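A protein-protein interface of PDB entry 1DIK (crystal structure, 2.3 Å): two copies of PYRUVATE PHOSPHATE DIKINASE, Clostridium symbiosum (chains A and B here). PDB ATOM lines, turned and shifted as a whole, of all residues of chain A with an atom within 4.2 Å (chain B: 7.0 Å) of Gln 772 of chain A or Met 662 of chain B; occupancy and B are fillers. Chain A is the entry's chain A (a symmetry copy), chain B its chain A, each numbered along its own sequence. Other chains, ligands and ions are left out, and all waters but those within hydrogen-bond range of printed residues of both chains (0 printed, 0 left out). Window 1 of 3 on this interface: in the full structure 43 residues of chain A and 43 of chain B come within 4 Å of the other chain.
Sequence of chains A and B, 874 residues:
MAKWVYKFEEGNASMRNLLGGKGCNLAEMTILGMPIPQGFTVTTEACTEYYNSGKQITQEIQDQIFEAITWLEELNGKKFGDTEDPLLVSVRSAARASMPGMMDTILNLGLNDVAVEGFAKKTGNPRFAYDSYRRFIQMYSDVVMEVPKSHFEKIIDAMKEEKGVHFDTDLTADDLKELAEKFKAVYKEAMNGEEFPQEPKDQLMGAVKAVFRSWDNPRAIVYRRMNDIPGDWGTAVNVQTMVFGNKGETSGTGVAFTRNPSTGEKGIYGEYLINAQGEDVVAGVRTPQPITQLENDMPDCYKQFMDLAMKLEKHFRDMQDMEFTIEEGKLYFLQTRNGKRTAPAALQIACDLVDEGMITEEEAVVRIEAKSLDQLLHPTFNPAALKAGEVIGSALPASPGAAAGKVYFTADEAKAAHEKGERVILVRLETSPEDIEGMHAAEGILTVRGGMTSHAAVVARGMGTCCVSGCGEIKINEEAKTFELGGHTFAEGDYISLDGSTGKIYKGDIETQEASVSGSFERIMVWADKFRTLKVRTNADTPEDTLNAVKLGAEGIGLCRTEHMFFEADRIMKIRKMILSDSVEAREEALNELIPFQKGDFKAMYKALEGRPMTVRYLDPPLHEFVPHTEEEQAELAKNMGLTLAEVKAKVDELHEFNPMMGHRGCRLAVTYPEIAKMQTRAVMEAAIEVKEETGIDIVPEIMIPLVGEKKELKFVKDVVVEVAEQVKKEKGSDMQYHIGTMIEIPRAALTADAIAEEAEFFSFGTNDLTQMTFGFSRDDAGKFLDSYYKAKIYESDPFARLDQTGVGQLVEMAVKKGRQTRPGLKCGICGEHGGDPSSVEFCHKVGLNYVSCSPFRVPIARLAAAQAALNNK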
ATOM      1  N   MET A 661      20.698 -37.483 -14.686  1.00  0.00           N
ATOM      2  CA  MET A 661      19.742 -37.612 -15.780  1.00  0.00           C
ATOM      3  C   MET A 661      20.461 -37.938 -17.090  1.00  0.00           C
ATOM      4  O   MET A 661      19.863 -38.324 -18.101  1.00  0.00           O
ATOM      5  CB  MET A 661      19.050 -36.269 -15.958  1.00  0.00           C
ATOM      6  CG  MET A 661      17.905 -36.312 -16.925  1.00  0.00           C
ATOM      7  SD  MET A 661      17.478 -34.681 -17.543  1.00  0.00           S
ATOM      8  CE  MET A 661      17.570 -34.968 -19.272  1.00  0.00           C
ATOM      9  N   MET A 662      21.767 -37.752 -17.059  1.00  0.00           N
ATOM     10  CA  MET A 662      22.581 -37.928 -18.240  1.00  0.00           C
ATOM     11  C   MET A 662      23.875 -38.688 -17.946  1.00  0.00           C
ATOM     12  O   MET A 662      24.881 -38.545 -18.646  1.00  0.00           O
ATOM     13  CB  MET A 662      22.897 -36.520 -18.816  1.00  0.00           C
ATOM     14  CG  MET A 662      21.813 -35.907 -19.675  1.00  0.00           C
ATOM     15  SD  MET A 662      22.438 -34.415 -20.414  1.00  0.00           S
ATOM     16  CE  MET A 662      22.879 -33.648 -18.795  1.00  0.00           C
ATOM     17  N   ASN A 768       8.727 -37.257 -21.941  1.00  0.00           N
ATOM     18  CA  ASN A 768       9.081 -36.479 -20.761  1.00  0.00           C
ATOM     19  C   ASN A 768      10.578 -36.181 -20.752  1.00  0.00           C
ATOM     20  O   ASN A 768      10.994 -35.041 -20.467  1.00  0.00           O
ATOM     21  CB  ASN A 768       8.714 -37.207 -19.464  1.00  0.00           C
ATOM     22  CG  ASN A 768       8.891 -36.320 -18.235  1.00  0.00           C
ATOM     23  OD1 ASN A 768       8.069 -35.410 -17.985  1.00  0.00           O
ATOM     24  ND2 ASN A 768       9.949 -36.556 -17.470  1.00  0.00           N
ATOM     25  N   ASP A 769      11.376 -37.233 -20.996  1.00  0.00           N
ATOM     26  CA  ASP A 769      12.833 -37.130 -21.035  1.00  0.00           C
ATOM     27  C   ASP A 769      13.317 -36.572 -22.368  1.00  0.00           C
ATOM     28  O   ASP A 769      14.317 -35.867 -22.395  1.00  0.00           O
ATOM     29  CB  ASP A 769      13.472 -38.480 -20.776  1.00  0.00           C
ATOM     30  CG  ASP A 769      12.739 -39.261 -19.724  1.00  0.00           C
ATOM     31  OD1 ASP A 769      13.060 -38.995 -18.537  1.00  0.00           O
ATOM     32  OD2 ASP A 769      11.827 -40.090 -20.102  1.00  0.00           O
ATOM     33  N   LEU A 770      12.621 -36.910 -23.448  1.00  0.00           N
ATOM     34  CA  LEU A 770      12.911 -36.397 -24.748  1.00  0.00           C
ATOM     35  C   LEU A 770      12.796 -34.874 -24.702  1.00  0.00           C
ATOM     36  O   LEU A 770      13.622 -34.191 -25.251  1.00  0.00           O
ATOM     37  CB  LEU A 770      11.941 -36.974 -25.770  1.00  0.00           C
ATOM     38  CG  LEU A 770      12.183 -36.529 -27.212  1.00  0.00           C
ATOM     39  CD1 LEU A 770      13.578 -36.833 -27.582  1.00  0.00           C
ATOM     40  CD2 LEU A 770      11.275 -37.173 -28.244  1.00  0.00           C
ATOM     41  N   THR A 771      11.776 -34.367 -24.013  1.00  0.00           N
ATOM     42  CA  THR A 771      11.477 -32.953 -23.840  1.00  0.00           C
ATOM     43  C   THR A 771      12.626 -32.375 -23.038  1.00  0.00           C
ATOM     44  O   THR A 771      13.164 -31.307 -23.349  1.00  0.00           O
ATOM     45  CB  THR A 771      10.140 -32.780 -23.039  1.00  0.00           C
ATOM     46  OG1 THR A 771       9.034 -33.063 -23.880  1.00  0.00           O
ATOM     47  CG2 THR A 771       9.988 -31.448 -22.521  1.00  0.00           C
ATOM     48  N   GLN A 772      12.948 -33.040 -21.944  1.00  0.00           N
ATOM     49  CA  GLN A 772      14.068 -32.629 -21.114  1.00  0.00           C
ATOM     50  C   GLN A 772      15.409 -32.460 -21.850  1.00  0.00           C
ATOM     51  O   GLN A 772      16.211 -31.626 -21.465  1.00  0.00           O
ATOM     52  CB  GLN A 772      14.238 -33.604 -19.951  1.00  0.00           C
ATOM     53  CG  GLN A 772      13.364 -33.230 -18.827  1.00  0.00           C
ATOM     54  CD  GLN A 772      13.390 -34.178 -17.680  1.00  0.00           C
ATOM     55  OE1 GLN A 772      14.213 -34.064 -16.785  1.00  0.00           O
ATOM     56  NE2 GLN A 772      12.406 -35.050 -17.626  1.00  0.00           N
ATOM     57  N   MET A 773      15.628 -33.170 -22.948  1.00  0.00           N
ATOM     58  CA  MET A 773      16.916 -33.051 -23.618  1.00  0.00           C
ATOM     59  C   MET A 773      16.893 -32.093 -24.780  1.00  0.00           C
ATOM     60  O   MET A 773      17.914 -31.557 -25.190  1.00  0.00           O
ATOM     61  CB  MET A 773      17.380 -34.419 -24.090  1.00  0.00           C
ATOM     62  CG  MET A 773      17.162 -35.514 -23.099  1.00  0.00           C
ATOM     63  SD  MET A 773      18.675 -36.380 -22.656  1.00  0.00           S
ATOM     64  CE  MET A 773      19.621 -34.944 -22.040  1.00  0.00           C
ATOM     65  N   THR A 774      15.709 -31.976 -25.352  1.00  0.00           N
ATOM     66  CA  THR A 774      15.433 -31.106 -26.471  1.00  0.00           C
ATOM     67  C   THR A 774      15.425 -29.668 -25.994  1.00  0.00           C
ATOM     68  O   THR A 774      15.866 -28.791 -26.717  1.00  0.00           O
ATOM     69  CB  THR A 774      14.079 -31.459 -27.043  1.00  0.00           C
ATOM     70  OG1 THR A 774      14.111 -32.820 -27.486  1.00  0.00           O
ATOM     71  CG2 THR A 774      13.629 -30.505 -28.156  1.00  0.00           C
ATOM     72  N   GLY A 776      16.616 -28.776 -22.805  1.00  0.00           N
ATOM     73  CA  GLY A 776      17.774 -28.340 -22.108  1.00  0.00           C
ATOM     74  C   GLY A 776      17.471 -28.203 -20.682  1.00  0.00           C
ATOM     75  O   GLY A 776      18.227 -27.588 -19.944  1.00  0.00           O
ATOM     76  N   PHE A 777      16.337 -28.694 -20.252  1.00  0.00           N
ATOM     77  CA  PHE A 777      16.143 -28.622 -18.828  1.00  0.00           C
ATOM     78  C   PHE A 777      15.538 -29.819 -18.160  1.00  0.00           C
ATOM     79  O   PHE A 777      14.776 -30.561 -18.759  1.00  0.00           O
ATOM     80  CB  PHE A 777      15.453 -27.332 -18.375  1.00  0.00           C
ATOM     81  CG  PHE A 777      14.246 -26.987 -19.131  1.00  0.00           C
ATOM     82  CD1 PHE A 777      13.157 -27.832 -19.140  1.00  0.00           C
ATOM     83  CD2 PHE A 777      14.188 -25.791 -19.807  1.00  0.00           C
ATOM     84  CE1 PHE A 777      11.979 -27.467 -19.831  1.00  0.00           C
ATOM     85  CE2 PHE A 777      13.054 -25.421 -20.482  1.00  0.00           C
ATOM     86  CZ  PHE A 777      11.938 -26.258 -20.498  1.00  0.00           C
ATOM     87  N   SER A 778      15.969 -30.012 -16.924  1.00  0.00           N
ATOM     88  CA  SER A 778      15.519 -31.080 -16.069  1.00  0.00           C
ATOM     89  C   SER A 778      14.232 -30.577 -15.499  1.00  0.00           C
ATOM     90  O   SER A 778      14.134 -29.421 -15.052  1.00  0.00           O
ATOM     91  CB  SER A 778      16.489 -31.301 -14.925  1.00  0.00           C
ATOM     92  OG  SER A 778      16.759 -30.090 -14.266  1.00  0.00           O
ATOM     93  N   ARG A 779      13.242 -31.452 -15.513  1.00  0.00           N
ATOM     94  CA  ARG A 779      11.936 -31.134 -15.022  1.00  0.00           C
ATOM     95  C   ARG A 779      12.056 -30.686 -13.561  1.00  0.00           C
ATOM     96  O   ARG A 779      11.437 -29.700 -13.135  1.00  0.00           O
ATOM     97  CB  ARG A 779      11.109 -32.377 -15.162  1.00  0.00           C
ATOM     98  CG  ARG A 779       9.650 -32.210 -14.893  1.00  0.00           C
ATOM     99  CD  ARG A 779       8.943 -33.494 -15.260  1.00  0.00           C
ATOM    100  NE  ARG A 779       7.714 -33.683 -14.514  1.00  0.00           N
ATOM    101  CZ  ARG A 779       6.537 -33.952 -15.065  1.00  0.00           C
ATOM    102  NH1 ARG A 779       6.404 -34.084 -16.384  1.00  0.00           N
ATOM    103  NH2 ARG A 779       5.484 -34.048 -14.275  1.00  0.00           N
ATOM    104  N   PHE A 800       6.005 -30.181 -20.147  1.00  0.00           N
ATOM    105  CA  PHE A 800       5.930 -31.481 -19.506  1.00  0.00           C
ATOM    106  C   PHE A 800       4.545 -32.103 -19.385  1.00  0.00           C
ATOM    107  O   PHE A 800       4.409 -33.275 -19.086  1.00  0.00           O
ATOM    108  CB  PHE A 800       6.536 -31.367 -18.142  1.00  0.00           C
ATOM    109  CG  PHE A 800       7.965 -31.040 -18.198  1.00  0.00           C
ATOM    110  CD1 PHE A 800       8.870 -31.973 -18.726  1.00  0.00           C
ATOM    111  CD2 PHE A 800       8.413 -29.795 -17.863  1.00  0.00           C
ATOM    112  CE1 PHE A 800      10.202 -31.664 -18.929  1.00  0.00           C
ATOM    113  CE2 PHE A 800       9.729 -29.469 -18.056  1.00  0.00           C
ATOM    114  CZ  PHE A 800      10.625 -30.417 -18.598  1.00  0.00           C
ATOM    115  N   PRO B 622      25.110 -21.795 -13.645  1.00  0.00           N
ATOM    116  CA  PRO B 622      24.099 -21.633 -12.613  1.00  0.00           C
ATOM    117  C   PRO B 622      24.740 -20.798 -11.497  1.00  0.00           C
ATOM    118  O   PRO B 622      25.945 -20.949 -11.204  1.00  0.00           O
ATOM    119  CB  PRO B 622      23.893 -23.059 -12.111  1.00  0.00           C
ATOM    120  CG  PRO B 622      24.487 -23.907 -13.095  1.00  0.00           C
ATOM    121  CD  PRO B 622      25.611 -23.181 -13.661  1.00  0.00           C
ATOM    122  N   GLU B 657      21.201 -27.808  -7.564  1.00  0.00           N
ATOM    123  CA  GLU B 657      20.413 -28.509  -8.548  1.00  0.00           C
ATOM    124  C   GLU B 657      20.876 -29.944  -8.704  1.00  0.00           C
ATOM    125  O   GLU B 657      22.041 -30.284  -8.462  1.00  0.00           O
ATOM    126  CB  GLU B 657      20.561 -27.828  -9.904  1.00  0.00           C
ATOM    127  CG  GLU B 657      19.853 -26.527 -10.036  1.00  0.00           C
ATOM    128  CD  GLU B 657      20.429 -25.648 -11.125  1.00  0.00           C
ATOM    129  OE1 GLU B 657      21.590 -25.838 -11.544  1.00  0.00           O
ATOM    130  OE2 GLU B 657      19.743 -24.699 -11.501  1.00  0.00           O
ATOM    131  N   ASN B 659      20.662 -31.589 -11.774  1.00  0.00           N
ATOM    132  CA  ASN B 659      21.344 -31.588 -13.066  1.00  0.00           C
ATOM    133  C   ASN B 659      21.709 -30.183 -13.507  1.00  0.00           C
ATOM    134  O   ASN B 659      20.997 -29.597 -14.313  1.00  0.00           O
ATOM    135  CB  ASN B 659      20.437 -32.204 -14.120  1.00  0.00           C
ATOM    136  CG  ASN B 659      20.253 -33.661 -13.920  1.00  0.00           C
ATOM    137  OD1 ASN B 659      21.007 -34.456 -14.447  1.00  0.00           O
ATOM    138  ND2 ASN B 659      19.253 -34.035 -13.168  1.00  0.00           N
ATOM    139  N   PRO B 660      22.799 -29.626 -12.949  1.00  0.00           N
ATOM    140  CA  PRO B 660      23.467 -28.317 -13.109  1.00  0.00           C
ATOM    141  C   PRO B 660      23.737 -27.884 -14.563  1.00  0.00           C
ATOM    142  O   PRO B 660      23.953 -26.686 -14.859  1.00  0.00           O
ATOM    143  CB  PRO B 660      24.761 -28.540 -12.352  1.00  0.00           C
ATOM    144  CG  PRO B 660      24.335 -29.376 -11.236  1.00  0.00           C
ATOM    145  CD  PRO B 660      23.450 -30.392 -11.873  1.00  0.00           C
ATOM    146  N   MET B 661      23.769 -28.879 -15.443  1.00  0.00           N
ATOM    147  CA  MET B 661      23.980 -28.707 -16.875  1.00  0.00           C
ATOM    148  C   MET B 661      22.670 -28.347 -17.576  1.00  0.00           C
ATOM    149  O   MET B 661      22.628 -27.923 -18.737  1.00  0.00           O
ATOM    150  CB  MET B 661      24.453 -30.037 -17.442  1.00  0.00           C
ATOM    151  CG  MET B 661      24.892 -29.953 -18.873  1.00  0.00           C
ATOM    152  SD  MET B 661      24.902 -31.560 -19.674  1.00  0.00           S
ATOM    153  CE  MET B 661      23.891 -31.219 -21.068  1.00  0.00           C
ATOM    154  N   MET B 662      21.587 -28.546 -16.849  1.00  0.00           N
ATOM    155  CA  MET B 662      20.264 -28.340 -17.394  1.00  0.00           C
ATOM    156  C   MET B 662      19.343 -27.602 -16.422  1.00  0.00           C
ATOM    157  O   MET B 662      18.117 -27.732 -16.470  1.00  0.00           O
ATOM    158  CB  MET B 662      19.674 -29.732 -17.751  1.00  0.00           C
ATOM    159  CG  MET B 662      20.114 -30.307 -19.079  1.00  0.00           C
ATOM    160  SD  MET B 662      19.175 -31.782 -19.408  1.00  0.00           S
ATOM    161  CE  MET B 662      19.674 -32.604 -17.833  1.00  0.00           C
ATOM    162  N   GLY B 663      19.936 -26.875 -15.498  1.00  0.00           N
ATOM    163  CA  GLY B 663      19.118 -26.137 -14.567  1.00  0.00           C
ATOM    164  C   GLY B 663      18.909 -24.663 -14.924  1.00  0.00           C
ATOM    165  O   GLY B 663      18.763 -24.273 -16.100  1.00  0.00           O
ATOM    166  N   HIS B 664      18.923 -23.839 -13.882  1.00  0.00           N
ATOM    167  CA  HIS B 664      18.720 -22.402 -13.972  1.00  0.00           C
ATOM    168  C   HIS B 664      20.014 -21.702 -14.319  1.00  0.00           C
ATOM    169  O   HIS B 664      20.708 -21.245 -13.422  1.00  0.00           O
ATOM    170  CB  HIS B 664      18.197 -21.890 -12.631  1.00  0.00           C
ATOM    171  CG  HIS B 664      17.610 -20.513 -12.717  1.00  0.00           C
ATOM    172  ND1 HIS B 664      17.223 -19.795 -11.606  1.00  0.00           N
ATOM    173  CD2 HIS B 664      17.350 -19.726 -13.784  1.00  0.00           C
ATOM    174  CE1 HIS B 664      16.746 -18.631 -11.986  1.00  0.00           C
ATOM    175  NE2 HIS B 664      16.815 -18.566 -13.304  1.00  0.00           N
ATOM    176  N   ARG B 665      20.301 -21.549 -15.609  1.00  0.00           N
ATOM    177  CA  ARG B 665      21.559 -20.948 -16.057  1.00  0.00           C
ATOM    178  C   ARG B 665      21.424 -20.391 -17.460  1.00  0.00           C
ATOM    179  O   ARG B 665      20.387 -20.556 -18.114  1.00  0.00           O
ATOM    180  CB  ARG B 665      22.684 -22.008 -16.088  1.00  0.00           C
ATOM    181  CG  ARG B 665      22.331 -23.125 -17.023  1.00  0.00           C
ATOM    182  CD  ARG B 665      23.471 -23.587 -17.870  1.00  0.00           C
ATOM    183  NE  ARG B 665      24.222 -24.571 -17.140  1.00  0.00           N
ATOM    184  CZ  ARG B 665      25.541 -24.681 -17.193  1.00  0.00           C
ATOM    185  NH1 ARG B 665      26.251 -23.873 -17.979  1.00  0.00           N
ATOM    186  NH2 ARG B 665      26.147 -25.546 -16.391  1.00  0.00           N
ATOM    187  N   ARG B 668      18.263 -18.372 -19.037  1.00  0.00           N
ATOM    188  CA  ARG B 668      17.288 -18.533 -17.958  1.00  0.00           C
ATOM    189  C   ARG B 668      17.447 -17.588 -16.781  1.00  0.00           C
ATOM    190  O   ARG B 668      16.465 -17.142 -16.227  1.00  0.00           O
ATOM    191  CB  ARG B 668      17.302 -19.976 -17.468  1.00  0.00           C
ATOM    192  CG  ARG B 668      16.774 -20.888 -18.508  1.00  0.00           C
ATOM    193  CD  ARG B 668      17.460 -22.168 -18.321  1.00  0.00           C
ATOM    194  NE  ARG B 668      17.547 -22.881 -19.576  1.00  0.00           N
ATOM    195  CZ  ARG B 668      17.696 -24.198 -19.637  1.00  0.00           C
ATOM    196  NH1 ARG B 668      17.774 -24.920 -18.532  1.00  0.00           N
ATOM    197  NH2 ARG B 668      17.676 -24.804 -20.781  1.00  0.00           N
ATOM    198  N   LEU B 707      22.389 -20.616 -24.265  1.00  0.00           N
ATOM    199  CA  LEU B 707      21.311 -21.574 -23.921  1.00  0.00           C
ATOM    200  C   LEU B 707      19.898 -21.320 -24.323  1.00  0.00           C
ATOM    201  O   LEU B 707      18.992 -21.632 -23.598  1.00  0.00           O
ATOM    202  CB  LEU B 707      21.294 -21.759 -22.410  1.00  0.00           C
ATOM    203  CG  LEU B 707      20.973 -23.153 -21.898  1.00  0.00           C
ATOM    204  CD1 LEU B 707      22.194 -24.060 -22.100  1.00  0.00           C
ATOM    205  CD2 LEU B 707      20.588 -23.098 -20.430  1.00  0.00           C
ATOM    206  N   PRO B 747      19.044 -28.722 -28.589  1.00  0.00           N
ATOM    207  CA  PRO B 747      18.416 -29.199 -29.808  1.00  0.00           C
ATOM    208  C   PRO B 747      17.217 -28.337 -30.281  1.00  0.00           C
ATOM    209  O   PRO B 747      17.101 -28.039 -31.462  1.00  0.00           O
ATOM    210  CB  PRO B 747      18.039 -30.650 -29.430  1.00  0.00           C
ATOM    211  CG  PRO B 747      19.000 -31.029 -28.438  1.00  0.00           C
ATOM    212  CD  PRO B 747      19.038 -29.796 -27.577  1.00  0.00           C
ATOM    213  N   GLN B 772      26.310 -33.019 -25.877  1.00  0.00           N
ATOM    214  CA  GLN B 772      25.815 -33.467 -24.586  1.00  0.00           C
ATOM    215  C   GLN B 772      24.287 -33.625 -24.483  1.00  0.00           C
ATOM    216  O   GLN B 772      23.814 -34.478 -23.752  1.00  0.00           O
ATOM    217  CB  GLN B 772      26.310 -32.530 -23.487  1.00  0.00           C
ATOM    218  CG  GLN B 772      27.651 -32.932 -23.027  1.00  0.00           C
ATOM    219  CD  GLN B 772      28.259 -32.021 -22.020  1.00  0.00           C
ATOM    220  OE1 GLN B 772      28.051 -32.170 -20.826  1.00  0.00           O
ATOM    221  NE2 GLN B 772      29.123 -31.141 -22.480  1.00  0.00           N
ATOM    222  N   MET B 773      23.515 -32.883 -25.265  1.00  0.00           N
ATOM    223  CA  MET B 773      22.068 -32.993 -25.134  1.00  0.00           C
ATOM    224  C   MET B 773      21.449 -33.913 -26.153  1.00  0.00           C
ATOM    225  O   MET B 773      20.364 -34.446 -25.960  1.00  0.00           O
ATOM    226  CB  MET B 773      21.436 -31.615 -25.236  1.00  0.00           C
ATOM    227  CG  MET B 773      22.165 -30.550 -24.487  1.00  0.00           C
ATOM    228  SD  MET B 773      21.141 -29.712 -23.268  1.00  0.00           S
ATOM    229  CE  MET B 773      20.667 -31.176 -22.283  1.00  0.00           C
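Gln 772 of chain A touches just one residue of chain B: Met 662 (3.6 Å). Of chain A, only Met 661 (3.0 Å), Met 662 (3.5 Å), Gln 772 (3.6 Å), Gly 776 (3.3 Å), Phe 777 (3.2 Å) and Ser 778 (3.2 Å) come within 4 Å of Met 662 of chain B. Of the printed residues of chain B, Met 661 of chain A touches Asn 659 (3.1 Å) and Met 662 (3.0 Å). Printed residues of chain A within 4 Å of Asn 659 of chain B: Met 661. Of the printed residues of chain B, Ser 778 of chain A touches Met 662 (3.2 Å). The nearest residue of chain B that does not touch Gln 772 of chain A is Met 773 of chain B (4.6 Å).
The backbone carbonyl oxygen of Gly 663 of chain B is in hydrogen-bond range of the guanidinium group of Arg 668 of chain B (2.7 Å). O of Arg 668 of chain B is in hydrogen-bond range of NE2 of His 664 of chain B, 3.3 Å away. The side-chain sulfur (SD) of Met 661 of chain A sits close to the side-chain amide oxygen (OE1) of Gln 772 of chain A, 3.4 Å away. The side-chain amide nitrogen (NE2) of Gln 772 of chain A sits close to the side-chain amide nitrogen (ND2) of Asn 768 of chain A. The backbone carbonyl oxygen (O) of Gln 772 of chain A lies within hydrogen-bond range of the backbone NH (N) of Phe 777 of chain A. The backbone NH (N) of Arg 779 of chain A is in hydrogen-bond range of the side-chain amide oxygen (OE1) of Gln 772 of chain A (3.1 Å).
Met 662 of chain B touches Met 661 of chain A (CE to SD, 3.0 Å). SD of Met 661 of chain B touches CE of Met 662 of chain A, 3.0 Å away. CE of Met 662 of chain B touches CE of Met 662 of chain A, 3.5 Å away. Pro 747 of chain B touches Met 773 of chain A. CB of Met 773 of chain A touches O of Met 773 of chain B (3.5 Å). Pro 747 of chain B touches Thr 774 of chain A (CD to O, 3.4 Å). SD of Met 773 of chain B touches CA of Gly 776 of chain A, 3.8 Å away. Phe 777 of chain A touches Met 662 of chain B (CA to O, 3.2 Å). Phe 777 of chain A touches Arg 668 of chain B.
The backbone NH of Met 661 of chain A sits at hydrogen-bond distance from the side-chain amide oxygen of Asn 659 of chain B (3.1 Å). O of Met 662 of chain B sits at hydrogen-bond distance from N of Ser 778 of chain A (3.2 Å). The guanidinium group (NH2) of Arg 668 of chain B sits at hydrogen-bond distance from the backbone carbonyl oxygen (O) of Gly 776 of chain A, at 3.0 Å. SD of Met 662 of chain A sits close to O of Gln 772 of chain B, 3.6 Å away. The backbone carbonyl oxygen (O) of Gln 772 of chain A sits close to the side-chain sulfur (SD) of Met 662 of chain B. O of Gly 776 of chain A sits close to O of Met 662 of chain B (3.5 Å).
Hydrophobic or aromatic side chains of chain A within 4 Å of the printed part of chain B: Met 661, Met 662, Met 773 and Phe 777. Of the 14 printed residues of chain B, 7 touch a printed residue of chain A. Hydrophobic or aromatic side chains of chain B that line the printed part of chain A: Met 661, Met 662, Pro 747 and Met 773. Among the printed residues, 15 pairs touch across the chains. Among the printed residues, no Asp or Glu carboxylate lies within 4 Å of a Lys or Arg side-chain nitrogen of the other chain.
Met 661 of chain A touches Met 662 of chain B, and with the chains exchanged Met 662 of chain A touches Met 661 of chain B. Met 662 of chain A touches its own counterpart, Met 662 of chain B. Met 662 of chain A touches Gln 772 of chain B, and with the chains exchanged Gln 772 of chain A touches Met 662 of chain B. Met 773 of chain B touches its own counterpart, Met 773 of chain A. Of the 15 pairs that touch across the chains among the printed residues, 6 have their exchanged pair printed and touching as well.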
